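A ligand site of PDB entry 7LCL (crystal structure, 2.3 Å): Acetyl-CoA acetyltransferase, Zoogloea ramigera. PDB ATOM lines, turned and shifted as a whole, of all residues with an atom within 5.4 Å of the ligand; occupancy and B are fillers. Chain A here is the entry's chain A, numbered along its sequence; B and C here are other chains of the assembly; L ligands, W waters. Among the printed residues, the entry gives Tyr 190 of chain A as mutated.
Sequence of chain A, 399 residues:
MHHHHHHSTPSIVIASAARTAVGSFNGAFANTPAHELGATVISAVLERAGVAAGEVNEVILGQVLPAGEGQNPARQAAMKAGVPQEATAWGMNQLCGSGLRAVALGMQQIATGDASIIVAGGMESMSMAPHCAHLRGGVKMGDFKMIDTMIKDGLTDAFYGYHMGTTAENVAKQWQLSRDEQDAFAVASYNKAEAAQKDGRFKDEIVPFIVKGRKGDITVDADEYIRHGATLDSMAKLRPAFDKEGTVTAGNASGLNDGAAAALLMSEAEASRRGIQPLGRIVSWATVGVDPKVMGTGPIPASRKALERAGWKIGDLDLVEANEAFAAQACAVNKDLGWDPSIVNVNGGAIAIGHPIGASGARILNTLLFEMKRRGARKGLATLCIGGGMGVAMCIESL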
ATOM      1  N   SCY A  96     -11.849 -18.104  32.307  1.00  0.00           N
ATOM      2  CA  SCY A  96     -11.960 -19.555  32.392  1.00  0.00           C
ATOM      3  CB  SCY A  96     -10.781 -20.151  33.123  1.00  0.00           C
ATOM      4  SG  SCY A  96      -9.265 -19.960  32.204  1.00  0.00           S
ATOM      5  CD  SCY A  96      -8.701 -18.379  32.481  1.00  0.00           C
ATOM      6  OCD SCY A  96      -8.853 -17.681  33.493  1.00  0.00           O
ATOM      7  CE  SCY A  96      -7.959 -17.872  31.282  1.00  0.00           C
ATOM      8  C   SCY A  96     -13.258 -20.099  33.091  1.00  0.00           C
ATOM      9  O   SCY A  96     -13.633 -21.283  32.850  1.00  0.00           O
ATOM     10  N   GLY A 154      -6.694 -13.394  26.725  1.00  0.00           N
ATOM     11  CA  GLY A 154      -7.049 -14.670  27.303  1.00  0.00           C
ATOM     12  C   GLY A 154      -6.045 -15.248  28.282  1.00  0.00           C
ATOM     13  O   GLY A 154      -6.436 -15.824  29.297  1.00  0.00           O
ATOM     14  N   LEU A 155      -4.747 -15.087  28.002  1.00  0.00           N
ATOM     15  CA  LEU A 155      -3.724 -15.800  28.747  1.00  0.00           C
ATOM     16  C   LEU A 155      -2.736 -14.902  29.490  1.00  0.00           C
ATOM     17  O   LEU A 155      -1.854 -15.433  30.169  1.00  0.00           O
ATOM     18  CB  LEU A 155      -2.947 -16.724  27.801  1.00  0.00           C
ATOM     19  CG  LEU A 155      -3.791 -17.678  26.957  1.00  0.00           C
ATOM     20  CD1 LEU A 155      -2.904 -18.528  26.054  1.00  0.00           C
ATOM     21  CD2 LEU A 155      -4.673 -18.555  27.831  1.00  0.00           C
ATOM     22  N   HIS A 163       2.268 -14.314  31.751  1.00  0.00           N
ATOM     23  CA  HIS A 163       1.342 -15.349  31.353  1.00  0.00           C
ATOM     24  C   HIS A 163       0.675 -15.986  32.579  1.00  0.00           C
ATOM     25  O   HIS A 163       1.139 -15.835  33.709  1.00  0.00           O
ATOM     26  CB  HIS A 163       2.069 -16.423  30.534  1.00  0.00           C
ATOM     27  CG  HIS A 163       1.168 -17.283  29.700  1.00  0.00           C
ATOM     28  ND1 HIS A 163       0.523 -18.389  30.204  1.00  0.00           N
ATOM     29  CD2 HIS A 163       0.824 -17.205  28.390  1.00  0.00           C
ATOM     30  CE1 HIS A 163      -0.193 -18.952  29.246  1.00  0.00           C
ATOM     31  NE2 HIS A 163      -0.026 -18.259  28.137  1.00  0.00           N
ATOM     32  N   MET A 164      -0.430 -16.689  32.333  1.00  0.00           N
ATOM     33  CA  MET A 164      -1.077 -17.450  33.388  1.00  0.00           C
ATOM     34  C   MET A 164      -0.169 -18.538  33.933  1.00  0.00           C
ATOM     35  O   MET A 164      -0.317 -18.946  35.093  1.00  0.00           O
ATOM     36  CB  MET A 164      -2.397 -18.053  32.879  1.00  0.00           C
ATOM     37  CG  MET A 164      -3.465 -17.034  32.501  1.00  0.00           C
ATOM     38  SD  MET A 164      -4.196 -16.178  33.910  1.00  0.00           S
ATOM     39  CE  MET A 164      -3.250 -14.661  33.934  1.00  0.00           C
ATOM     40  N   GLY A 165       0.756 -19.036  33.118  1.00  0.00           N
ATOM     41  CA  GLY A 165       1.712 -20.017  33.594  1.00  0.00           C
ATOM     42  C   GLY A 165       2.637 -19.484  34.669  1.00  0.00           C
ATOM     43  O   GLY A 165       3.113 -20.239  35.516  1.00  0.00           O
ATOM     44  N   TYR A 190      -3.182 -37.768  32.402  1.00  0.00           N
ATOM     45  CA  TYR A 190      -3.124 -38.381  31.071  1.00  0.00           C
ATOM     46  C   TYR A 190      -3.658 -39.807  31.096  1.00  0.00           C
ATOM     47  O   TYR A 190      -4.396 -40.210  30.201  1.00  0.00           O
ATOM     48  CB  TYR A 190      -1.695 -38.365  30.538  1.00  0.00           C
ATOM     49  CG  TYR A 190      -1.159 -36.996  30.167  1.00  0.00           C
ATOM     50  CD1 TYR A 190      -1.735 -36.253  29.158  1.00  0.00           C
ATOM     51  CD2 TYR A 190      -0.062 -36.455  30.839  1.00  0.00           C
ATOM     52  CE1 TYR A 190      -1.245 -35.001  28.811  1.00  0.00           C
ATOM     53  CE2 TYR A 190       0.428 -35.210  30.504  1.00  0.00           C
ATOM     54  CZ  TYR A 190      -0.167 -34.481  29.488  1.00  0.00           C
ATOM     55  OH  TYR A 190       0.327 -33.250  29.154  1.00  0.00           O
ATOM     56  N   TYR A 225      -6.967 -34.116  21.701  1.00  0.00           N
ATOM     57  CA  TYR A 225      -5.833 -33.689  22.496  1.00  0.00           C
ATOM     58  C   TYR A 225      -5.407 -34.724  23.536  1.00  0.00           C
ATOM     59  O   TYR A 225      -4.336 -34.582  24.135  1.00  0.00           O
ATOM     60  CB  TYR A 225      -6.150 -32.357  23.191  1.00  0.00           C
ATOM     61  CG  TYR A 225      -4.964 -31.720  23.877  1.00  0.00           C
ATOM     62  CD1 TYR A 225      -3.891 -31.220  23.141  1.00  0.00           C
ATOM     63  CD2 TYR A 225      -4.915 -31.590  25.261  1.00  0.00           C
ATOM     64  CE1 TYR A 225      -2.811 -30.628  23.751  1.00  0.00           C
ATOM     65  CE2 TYR A 225      -3.836 -31.005  25.884  1.00  0.00           C
ATOM     66  CZ  TYR A 225      -2.790 -30.523  25.130  1.00  0.00           C
ATOM     67  OH  TYR A 225      -1.711 -29.938  25.753  1.00  0.00           O
ATOM     68  N   ARG A 227      -3.606 -37.603  25.034  1.00  0.00           N
ATOM     69  CA  ARG A 227      -2.364 -38.290  24.678  1.00  0.00           C
ATOM     70  C   ARG A 227      -2.434 -39.745  25.092  1.00  0.00           C
ATOM     71  O   ARG A 227      -3.020 -40.094  26.114  1.00  0.00           O
ATOM     72  CB  ARG A 227      -1.174 -37.600  25.352  1.00  0.00           C
ATOM     73  CG  ARG A 227       0.190 -38.091  24.896  1.00  0.00           C
ATOM     74  CD  ARG A 227       1.294 -37.301  25.583  1.00  0.00           C
ATOM     75  NE  ARG A 227       1.510 -36.005  24.956  1.00  0.00           N
ATOM     76  CZ  ARG A 227       2.396 -35.773  23.990  1.00  0.00           C
ATOM     77  NH1 ARG A 227       3.158 -36.769  23.544  1.00  0.00           N
ATOM     78  NH2 ARG A 227       2.532 -34.564  23.475  1.00  0.00           N
ATOM     79  N   ALA A 230       1.489 -41.656  27.773  1.00  0.00           N
ATOM     80  CA  ALA A 230       2.371 -40.607  28.274  1.00  0.00           C
ATOM     81  C   ALA A 230       3.391 -41.203  29.235  1.00  0.00           C
ATOM     82  O   ALA A 230       3.038 -41.999  30.115  1.00  0.00           O
ATOM     83  CB  ALA A 230       1.562 -39.507  28.961  1.00  0.00           C
ATOM     84  N   THR A 231       4.658 -40.821  29.083  1.00  0.00           N
ATOM     85  CA  THR A 231       5.747 -41.361  29.883  1.00  0.00           C
ATOM     86  C   THR A 231       6.327 -40.273  30.770  1.00  0.00           C
ATOM     87  O   THR A 231       6.461 -39.117  30.355  1.00  0.00           O
ATOM     88  CB  THR A 231       6.848 -41.948  28.991  1.00  0.00           C
ATOM     89  OG1 THR A 231       7.686 -40.898  28.509  1.00  0.00           O
ATOM     90  CG2 THR A 231       6.232 -42.664  27.791  1.00  0.00           C
ATOM     91  N   SER A 234       9.871 -38.800  29.359  1.00  0.00           N
ATOM     92  CA  SER A 234       9.805 -37.831  28.275  1.00  0.00           C
ATOM     93  C   SER A 234       9.304 -36.474  28.762  1.00  0.00           C
ATOM     94  O   SER A 234       9.664 -35.441  28.196  1.00  0.00           O
ATOM     95  CB  SER A 234       8.929 -38.345  27.139  1.00  0.00           C
ATOM     96  OG  SER A 234       7.577 -38.484  27.558  1.00  0.00           O
ATOM     97  N   MET A 235       8.466 -36.470  29.809  1.00  0.00           N
ATOM     98  CA  MET A 235       7.979 -35.216  30.369  1.00  0.00           C
ATOM     99  C   MET A 235       9.033 -34.535  31.237  1.00  0.00           C
ATOM    100  O   MET A 235       9.013 -33.307  31.366  1.00  0.00           O
ATOM    101  CB  MET A 235       6.708 -35.462  31.175  1.00  0.00           C
ATOM    102  CG  MET A 235       5.556 -35.993  30.362  1.00  0.00           C
ATOM    103  SD  MET A 235       4.091 -36.319  31.370  1.00  0.00           S
ATOM    104  CE  MET A 235       3.886 -34.736  32.171  1.00  0.00           C
ATOM    105  N   LEU A 238      11.250 -32.122  29.167  1.00  0.00           N
ATOM    106  CA  LEU A 238      10.674 -30.905  28.601  1.00  0.00           C
ATOM    107  C   LEU A 238      11.211 -29.678  29.321  1.00  0.00           C
ATOM    108  O   LEU A 238      11.348 -29.663  30.548  1.00  0.00           O
ATOM    109  CB  LEU A 238       9.151 -30.942  28.687  1.00  0.00           C
ATOM    110  CG  LEU A 238       8.425 -32.061  27.933  1.00  0.00           C
ATOM    111  CD1 LEU A 238       6.924 -31.950  28.123  1.00  0.00           C
ATOM    112  CD2 LEU A 238       8.784 -32.021  26.456  1.00  0.00           C
ATOM    113  N   ALA A 241       8.182 -23.733  30.135  1.00  0.00           N
ATOM    114  CA  ALA A 241       7.608 -22.926  29.073  1.00  0.00           C
ATOM    115  C   ALA A 241       7.456 -21.451  29.422  1.00  0.00           C
ATOM    116  O   ALA A 241       7.122 -20.660  28.542  1.00  0.00           O
ATOM    117  CB  ALA A 241       6.249 -23.491  28.665  1.00  0.00           C
ATOM    118  N   PHE A 242       7.694 -21.068  30.675  1.00  0.00           N
ATOM    119  CA  PHE A 242       7.475 -19.685  31.077  1.00  0.00           C
ATOM    120  C   PHE A 242       8.680 -19.113  31.808  1.00  0.00           C
ATOM    121  O   PHE A 242       9.219 -18.072  31.412  1.00  0.00           O
ATOM    122  CB  PHE A 242       6.218 -19.581  31.945  1.00  0.00           C
ATOM    123  CG  PHE A 242       5.000 -20.196  31.319  1.00  0.00           C
ATOM    124  CD1 PHE A 242       4.289 -19.516  30.345  1.00  0.00           C
ATOM    125  CD2 PHE A 242       4.581 -21.468  31.688  1.00  0.00           C
ATOM    126  CE1 PHE A 242       3.173 -20.088  29.761  1.00  0.00           C
ATOM    127  CE2 PHE A 242       3.460 -22.033  31.115  1.00  0.00           C
ATOM    128  CZ  PHE A 242       2.751 -21.345  30.147  1.00  0.00           C
ATOM    129  N   THR A 249       5.765 -26.795  32.758  1.00  0.00           N
ATOM    130  CA  THR A 249       6.105 -27.105  31.372  1.00  0.00           C
ATOM    131  C   THR A 249       4.830 -27.354  30.582  1.00  0.00           C
ATOM    132  O   THR A 249       3.715 -27.306  31.116  1.00  0.00           O
ATOM    133  CB  THR A 249       7.031 -28.315  31.296  1.00  0.00           C
ATOM    134  OG1 THR A 249       6.308 -29.490  31.689  1.00  0.00           O
ATOM    135  CG2 THR A 249       8.237 -28.141  32.214  1.00  0.00           C
ATOM    136  N   ALA A 250       5.000 -27.617  29.283  1.00  0.00           N
ATOM    137  CA  ALA A 250       3.859 -27.959  28.444  1.00  0.00           C
ATOM    138  C   ALA A 250       3.238 -29.294  28.840  1.00  0.00           C
ATOM    139  O   ALA A 250       2.054 -29.527  28.551  1.00  0.00           O
ATOM    140  CB  ALA A 250       4.274 -27.998  26.975  1.00  0.00           C
ATOM    141  N   GLY A 251       3.994 -30.173  29.489  1.00  0.00           N
ATOM    142  CA  GLY A 251       3.495 -31.460  29.905  1.00  0.00           C
ATOM    143  C   GLY A 251       2.576 -31.405  31.115  1.00  0.00           C
ATOM    144  O   GLY A 251       1.563 -32.098  31.167  1.00  0.00           O
ATOM    145  N   ALA A 253       0.934 -28.701  32.118  1.00  0.00           N
ATOM    146  CA  ALA A 253       0.015 -27.584  31.975  1.00  0.00           C
ATOM    147  C   ALA A 253      -1.037 -27.925  30.938  1.00  0.00           C
ATOM    148  O   ALA A 253      -0.822 -28.751  30.041  1.00  0.00           O
ATOM    149  CB  ALA A 253       0.743 -26.289  31.576  1.00  0.00           C
ATOM    150  N   SER A 254      -2.188 -27.275  31.058  1.00  0.00           N
ATOM    151  CA  SER A 254      -3.247 -27.444  30.074  1.00  0.00           C
ATOM    152  C   SER A 254      -2.817 -26.838  28.730  1.00  0.00           C
ATOM    153  O   SER A 254      -1.889 -26.025  28.653  1.00  0.00           O
ATOM    154  CB  SER A 254      -4.542 -26.788  30.557  1.00  0.00           C
ATOM    155  OG  SER A 254      -4.371 -25.397  30.763  1.00  0.00           O
ATOM    156  N   GLY A 255      -3.502 -27.248  27.671  1.00  0.00           N
ATOM    157  CA  GLY A 255      -3.195 -26.800  26.335  1.00  0.00           C
ATOM    158  C   GLY A 255      -4.150 -25.716  25.843  1.00  0.00           C
ATOM    159  O   GLY A 255      -5.028 -25.224  26.559  1.00  0.00           O
ATOM    160  N   LEU A 256      -3.946 -25.341  24.586  1.00  0.00           N
ATOM    161  CA  LEU A 256      -4.829 -24.417  23.878  1.00  0.00           C
ATOM    162  C   LEU A 256      -5.765 -25.246  23.004  1.00  0.00           C
ATOM    163  O   LEU A 256      -5.296 -26.053  22.197  1.00  0.00           O
ATOM    164  CB  LEU A 256      -4.014 -23.434  23.037  1.00  0.00           C
ATOM    165  CG  LEU A 256      -2.781 -22.848  23.729  1.00  0.00           C
ATOM    166  CD1 LEU A 256      -1.967 -22.006  22.762  1.00  0.00           C
ATOM    167  CD2 LEU A 256      -3.185 -22.040  24.949  1.00  0.00           C
ATOM    168  N   MET A 295      -3.903 -16.706  41.021  1.00  0.00           N
ATOM    169  CA  MET A 295      -5.289 -16.938  40.600  1.00  0.00           C
ATOM    170  C   MET A 295      -5.673 -18.412  40.635  1.00  0.00           C
ATOM    171  O   MET A 295      -6.864 -18.722  40.723  1.00  0.00           O
ATOM    172  CB  MET A 295      -5.509 -16.373  39.196  1.00  0.00           C
ATOM    173  CG  MET A 295      -4.691 -17.055  38.109  1.00  0.00           C
ATOM    174  SD  MET A 295      -5.541 -18.459  37.359  1.00  0.00           S
ATOM    175  CE  MET A 295      -4.169 -19.316  36.583  1.00  0.00           C
ATOM    176  N   ALA A 325      -6.096 -26.365  35.039  1.00  0.00           N
ATOM    177  CA  ALA A 325      -5.409 -25.336  34.269  1.00  0.00           C
ATOM    178  C   ALA A 325      -3.904 -25.535  34.321  1.00  0.00           C
ATOM    179  O   ALA A 325      -3.208 -25.411  33.308  1.00  0.00           O
ATOM    180  CB  ALA A 325      -5.799 -23.950  34.774  1.00  0.00           C
ATOM    181  N   PHE A 326      -3.378 -25.845  35.508  1.00  0.00           N
ATOM    182  CA  PHE A 326      -1.975 -26.165  35.685  1.00  0.00           C
ATOM    183  C   PHE A 326      -1.860 -27.214  36.783  1.00  0.00           C
ATOM    184  O   PHE A 326      -2.657 -27.234  37.722  1.00  0.00           O
ATOM    185  CB  PHE A 326      -1.132 -24.929  36.038  1.00  0.00           C
ATOM    186  CG  PHE A 326      -1.143 -23.866  34.990  1.00  0.00           C
ATOM    187  CD1 PHE A 326      -0.229 -23.890  33.941  1.00  0.00           C
ATOM    188  CD2 PHE A 326      -2.064 -22.835  35.025  1.00  0.00           C
ATOM    189  CE1 PHE A 326      -0.239 -22.919  32.972  1.00  0.00           C
ATOM    190  CE2 PHE A 326      -2.078 -21.850  34.055  1.00  0.00           C
ATOM    191  CZ  PHE A 326      -1.167 -21.896  33.026  1.00  0.00           C
ATOM    192  N   HIS A 355      -8.299 -27.459  27.351  1.00  0.00           N
ATOM    193  CA  HIS A 355      -8.771 -26.278  28.081  1.00  0.00           C
ATOM    194  C   HIS A 355      -9.230 -25.205  27.117  1.00  0.00           C
ATOM    195  O   HIS A 355      -8.510 -24.232  26.857  1.00  0.00           O
ATOM    196  CB  HIS A 355      -7.679 -25.752  29.018  1.00  0.00           C
ATOM    197  CG  HIS A 355      -8.151 -24.708  29.972  1.00  0.00           C
ATOM    198  ND1 HIS A 355      -9.485 -24.396  30.138  1.00  0.00           N
ATOM    199  CD2 HIS A 355      -7.464 -23.893  30.808  1.00  0.00           C
ATOM    200  CE1 HIS A 355      -9.602 -23.434  31.038  1.00  0.00           C
ATOM    201  NE2 HIS A 355      -8.391 -23.109  31.466  1.00  0.00           N
ATOM    202  N   ILE A 357     -11.021 -22.094  27.051  1.00  0.00           N
ATOM    203  CA  ILE A 357     -11.251 -21.241  28.228  1.00  0.00           C
ATOM    204  C   ILE A 357     -12.738 -20.940  28.408  1.00  0.00           C
ATOM    205  O   ILE A 357     -13.331 -21.229  29.454  1.00  0.00           O
ATOM    206  CB  ILE A 357     -10.421 -19.954  28.132  1.00  0.00           C
ATOM    207  CG1 ILE A 357     -10.412 -19.398  26.712  1.00  0.00           C
ATOM    208  CG2 ILE A 357      -8.996 -20.213  28.593  1.00  0.00           C
ATOM    209  CD1 ILE A 357      -9.509 -18.198  26.522  1.00  0.00           C
ATOM    210  N   CYS A 385     -10.467 -22.257  38.280  1.00  0.00           N
ATOM    211  CA  CYS A 385      -9.749 -21.028  38.562  1.00  0.00           C
ATOM    212  C   CYS A 385      -9.929 -20.048  37.409  1.00  0.00           C
ATOM    213  O   CYS A 385     -10.132 -20.451  36.259  1.00  0.00           O
ATOM    214  CB  CYS A 385      -8.263 -21.296  38.793  1.00  0.00           C
ATOM    215  SG  CYS A 385      -7.390 -21.967  37.359  1.00  0.00           S
ATOM    216  N   GLY A 387      -8.505 -16.340  35.600  1.00  0.00           N
ATOM    217  CA  GLY A 387      -7.455 -15.340  35.506  1.00  0.00           C
ATOM    218  C   GLY A 387      -7.893 -14.009  36.093  1.00  0.00           C
ATOM    219  O   GLY A 387      -9.078 -13.684  36.181  1.00  0.00           O
ATOM    220  N   MET B 141       1.373 -18.644  17.190  1.00  0.00           N
ATOM    221  CA  MET B 141       1.196 -18.105  18.527  1.00  0.00           C
ATOM    222  C   MET B 141       2.118 -16.912  18.745  1.00  0.00           C
ATOM    223  O   MET B 141       3.233 -16.869  18.220  1.00  0.00           O
ATOM    224  CB  MET B 141       1.465 -19.174  19.601  1.00  0.00           C
ATOM    225  CG  MET B 141       0.990 -18.810  20.981  1.00  0.00           C
ATOM    226  SD  MET B 141       1.493 -20.016  22.228  1.00  0.00           S
ATOM    227  CE  MET B 141       1.952 -21.411  21.212  1.00  0.00           C
ATOM    228  N   LYS C 215      16.350 -27.836  13.891  1.00  0.00           N
ATOM    229  CA  LYS C 215      16.372 -29.285  14.053  1.00  0.00           C
ATOM    230  C   LYS C 215      17.377 -29.949  13.116  1.00  0.00           C
ATOM    231  O   LYS C 215      17.203 -31.114  12.736  1.00  0.00           O
ATOM    232  CB  LYS C 215      14.985 -29.861  13.831  1.00  0.00           C
ATOM    233  CG  LYS C 215      13.952 -29.386  14.849  1.00  0.00           C
ATOM    234  CD  LYS C 215      12.542 -29.759  14.439  1.00  0.00           C
ATOM    235  CE  LYS C 215      11.527 -29.228  15.432  1.00  0.00           C
ATOM    236  NZ  LYS C 215      10.125 -29.445  14.971  1.00  0.00           N
HETATM  237  N1  LIG L   1       4.747 -35.419  27.195  1.00  0.00           N
HETATM  238  C1  LIG L   1       5.726 -35.330  26.314  1.00  0.00           C
HETATM  239  N2  LIG L   1       5.837 -34.311  25.494  1.00  0.00           N
HETATM  240  C2  LIG L   1       4.951 -33.315  25.511  1.00  0.00           C
HETATM  241  C3  LIG L   1       3.897 -33.373  26.440  1.00  0.00           C
HETATM  242  C4  LIG L   1       3.820 -34.483  27.299  1.00  0.00           C
HETATM  243  N3  LIG L   1       2.790 -34.593  28.224  1.00  0.00           N
HETATM  244  N4  LIG L   1       3.155 -32.260  26.257  1.00  0.00           N
HETATM  245  C5  LIG L   1       3.667 -31.536  25.317  1.00  0.00           C
HETATM  246  N5  LIG L   1       4.782 -32.146  24.823  1.00  0.00           N
HETATM  247  C6  LIG L   1       5.641 -31.632  23.744  1.00  0.00           C
HETATM  248  C7  LIG L   1       4.932 -31.690  22.377  1.00  0.00           C
HETATM  249  O1  LIG L   1       4.952 -33.012  21.818  1.00  0.00           O
HETATM  250  C8  LIG L   1       5.834 -30.729  21.574  1.00  0.00           C
HETATM  251  O2  LIG L   1       7.053 -31.406  21.255  1.00  0.00           O
HETATM  252  P1  LIG L   1       7.651 -30.762  19.903  1.00  0.00           P
HETATM  253  O3  LIG L   1       8.081 -29.367  20.140  1.00  0.00           O
HETATM  254  O4  LIG L   1       8.919 -31.635  19.422  1.00  0.00           O
HETATM  255  O5  LIG L   1       6.519 -30.793  18.751  1.00  0.00           O
HETATM  256  C9  LIG L   1       6.069 -29.630  22.620  1.00  0.00           C
HETATM  257  O6  LIG L   1       5.895 -30.216  23.924  1.00  0.00           O
HETATM  258  C10 LIG L   1       5.078 -28.473  22.400  1.00  0.00           C
HETATM  259  O7  LIG L   1       3.926 -28.628  23.234  1.00  0.00           O
HETATM  260  P2  LIG L   1       2.648 -28.129  22.392  1.00  0.00           P
HETATM  261  O8  LIG L   1       1.416 -28.564  23.071  1.00  0.00           O
HETATM  262  O9  LIG L   1       2.690 -28.822  20.936  1.00  0.00           O
HETATM  263  O10 LIG L   1       2.726 -26.534  22.167  1.00  0.00           O
HETATM  264  P3  LIG L   1       1.778 -25.626  23.124  1.00  0.00           P
HETATM  265  O11 LIG L   1       1.642 -24.320  22.448  1.00  0.00           O
HETATM  266  O12 LIG L   1       0.294 -26.216  23.320  1.00  0.00           O
HETATM  267  O13 LIG L   1       2.457 -25.410  24.561  1.00  0.00           O
HETATM  268  C11 LIG L   1       1.956 -23.566  26.086  1.00  0.00           C
HETATM  269  C12 LIG L   1       2.580 -23.998  24.753  1.00  0.00           C
HETATM  270  C13 LIG L   1       2.380 -24.538  27.184  1.00  0.00           C
HETATM  271  C14 LIG L   1       2.498 -22.168  26.408  1.00  0.00           C
HETATM  272  C15 LIG L   1       0.430 -23.550  25.950  1.00  0.00           C
HETATM  273  O14 LIG L   1      -0.026 -24.913  25.883  1.00  0.00           O
HETATM  274  C16 LIG L   1      -0.285 -22.854  27.087  1.00  0.00           C
HETATM  275  O15 LIG L   1      -0.365 -21.651  27.121  1.00  0.00           O
HETATM  276  N6  LIG L   1      -0.865 -23.575  28.076  1.00  0.00           N
HETATM  277  C17 LIG L   1      -1.560 -22.897  29.171  1.00  0.00           C
HETATM  278  C18 LIG L   1      -3.007 -22.581  28.789  1.00  0.00           C
HETATM  279  C19 LIG L   1      -3.612 -21.628  29.787  1.00  0.00           C
HETATM  280  O16 LIG L   1      -2.911 -20.825  30.359  1.00  0.00           O
HETATM  281  N7  LIG L   1      -4.928 -21.676  30.063  1.00  0.00           N
HETATM  282  C20 LIG L   1      -5.521 -20.757  31.051  1.00  0.00           C
HETATM  283  C21 LIG L   1      -5.201 -21.268  32.454  1.00  0.00           C
HETATM  284  S1  LIG L   1      -6.101 -20.276  33.684  1.00  0.00           S
HETATM  285  O   HOH W   1       8.305 -34.724  24.048  1.00  0.00           O
HETATM  286  O   HOH W   2       1.049 -19.284  25.701  1.00  0.00           O
HETATM  287  O   HOH W   3      -5.981 -22.870  27.241  1.00  0.00           O
HETATM  288  O   HOH W   4       0.148 -27.822  27.145  1.00  0.00           O
HETATM  289  O   HOH W   5       4.868 -36.268  21.066  1.00  0.00           O
HETATM  290  O   HOH W   6       9.366 -33.098  22.468  1.00  0.00           O
HETATM  291  O   HOH W   7       0.575 -31.381  27.149  1.00  0.00           O
HETATM  292  O   HOH W   8       5.130 -24.628  22.740  1.00  0.00           O
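The backbone carbonyl oxygen of Ser 254 sits at hydrogen-bond distance from a nitrogen (N6) of the ligand, at 2.7 Å. OH of Tyr 190 sits at hydrogen-bond distance from N3 of the ligand (3.0 Å). S1 of the ligand lies close to SG of SCY 96 (3.5 Å). The guanidinium group (NH2) of Arg 227 lies within hydrogen-bond range of an oxygen (O1) of the ligand (3.3 Å).
Water W7 lies within hydrogen-bond range of the side-chain hydroxyl of Tyr 190 (2.8 Å), the backbone carbonyl oxygen of Ala 250 (2.8 Å), a nitrogen (N4) of the ligand (2.9 Å) and the side-chain hydroxyl of Tyr 225 (3.0 Å). Water W2 lies within hydrogen-bond range of NE2 of His 163 (2.9 Å), O15 of the ligand (3.1 Å) and SD of Met 141 of chain B (3.6 Å). Water W3 lies within hydrogen-bond range of O of Gly 255 (2.6 Å), O of His 355 (2.9 Å) and N7 of the ligand (3.2 Å). Water W5 lies within hydrogen-bond range of the guanidinium group (NH1) of Arg 227 (3.1 Å) and an oxygen (O1) of the ligand (3.3 Å).
The side-chain hydroxyl of Ser 254 lies within hydrogen-bond range of the backbone carbonyl oxygen of Ala 325, at 2.8 Å. The backbone NH (N) of Met 164 is in hydrogen-bond range of the backbone carbonyl oxygen (O) of Leu 155, at 2.9 Å. A ring nitrogen (ND1) of His 163 lies within hydrogen-bond range of the backbone NH (N) of Gly 165 (3.0 Å). SG of SCY 96 lies within hydrogen-bond range of NE2 of His 355 (3.4 Å). The backbone NH (N) of Gly 251 sits close to the side-chain hydroxyl (OG1) of Thr 249, 3.3 Å away. OCD of SCY 96 lies within hydrogen-bond range of N of Gly 387, 2.5 Å away. OG of Ser 234 is in hydrogen-bond range of OG1 of Thr 231 (2.6 Å). The backbone carbonyl oxygen (O) of Gly 251 sits at hydrogen-bond distance from the side-chain hydroxyl (OH) of Tyr 190 (2.6 Å).
Leu 155 touches the ligand (CD2 to C19, 3.8 Å). His 163 touches the ligand (CE1 to O15, 3.4 Å). Met 164 touches the ligand. Ser 234 touches the ligand. Met 235 touches the ligand (CG to N1, 3.3 Å). CD1 of Leu 238 touches C2 of the ligand, 3.5 Å away. Phe 242 touches the ligand. Ala 250 touches the ligand. CA of Gly 251 touches N3 of the ligand, 3.6 Å away. Gly 255 touches the ligand. Leu 256 touches the ligand (CD2 to O15, 3.6 Å). CE of Met 295 touches S1 of the ligand (3.6 Å). Ala 325 touches the ligand (CB to C21, 3.6 Å). Phe 326 touches the ligand (CZ to O16, 3.4 Å). His 355 touches the ligand. Met 141 of chain B touches the ligand. Hydrophobic or aromatic side chains within 4 Å of the ligand: Leu 155, His 163, Met 164, Tyr 190, Met 235, Leu 238, Phe 242, Ala 250, Leu 256, Met 295, Ala 325, Phe 326, His 355 and Met 141 of chain B. Within 4 Å of the ligand: SCY 96, Leu 155, His 163, Met 164, Tyr 190, Arg 227, Ser 234, Met 235, Leu 238, Phe 242, Ala 250, Gly 251, Ser 254, Gly 255, Leu 256, Met 295, Ala 325, Phe 326, His 355 and Met 141 of chain B. Along chain A the residues within 4 Å of the ligand span positions 96 to 355. The nearest printed residue that does not touch the ligand is Cys 385 (4.2 Å).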
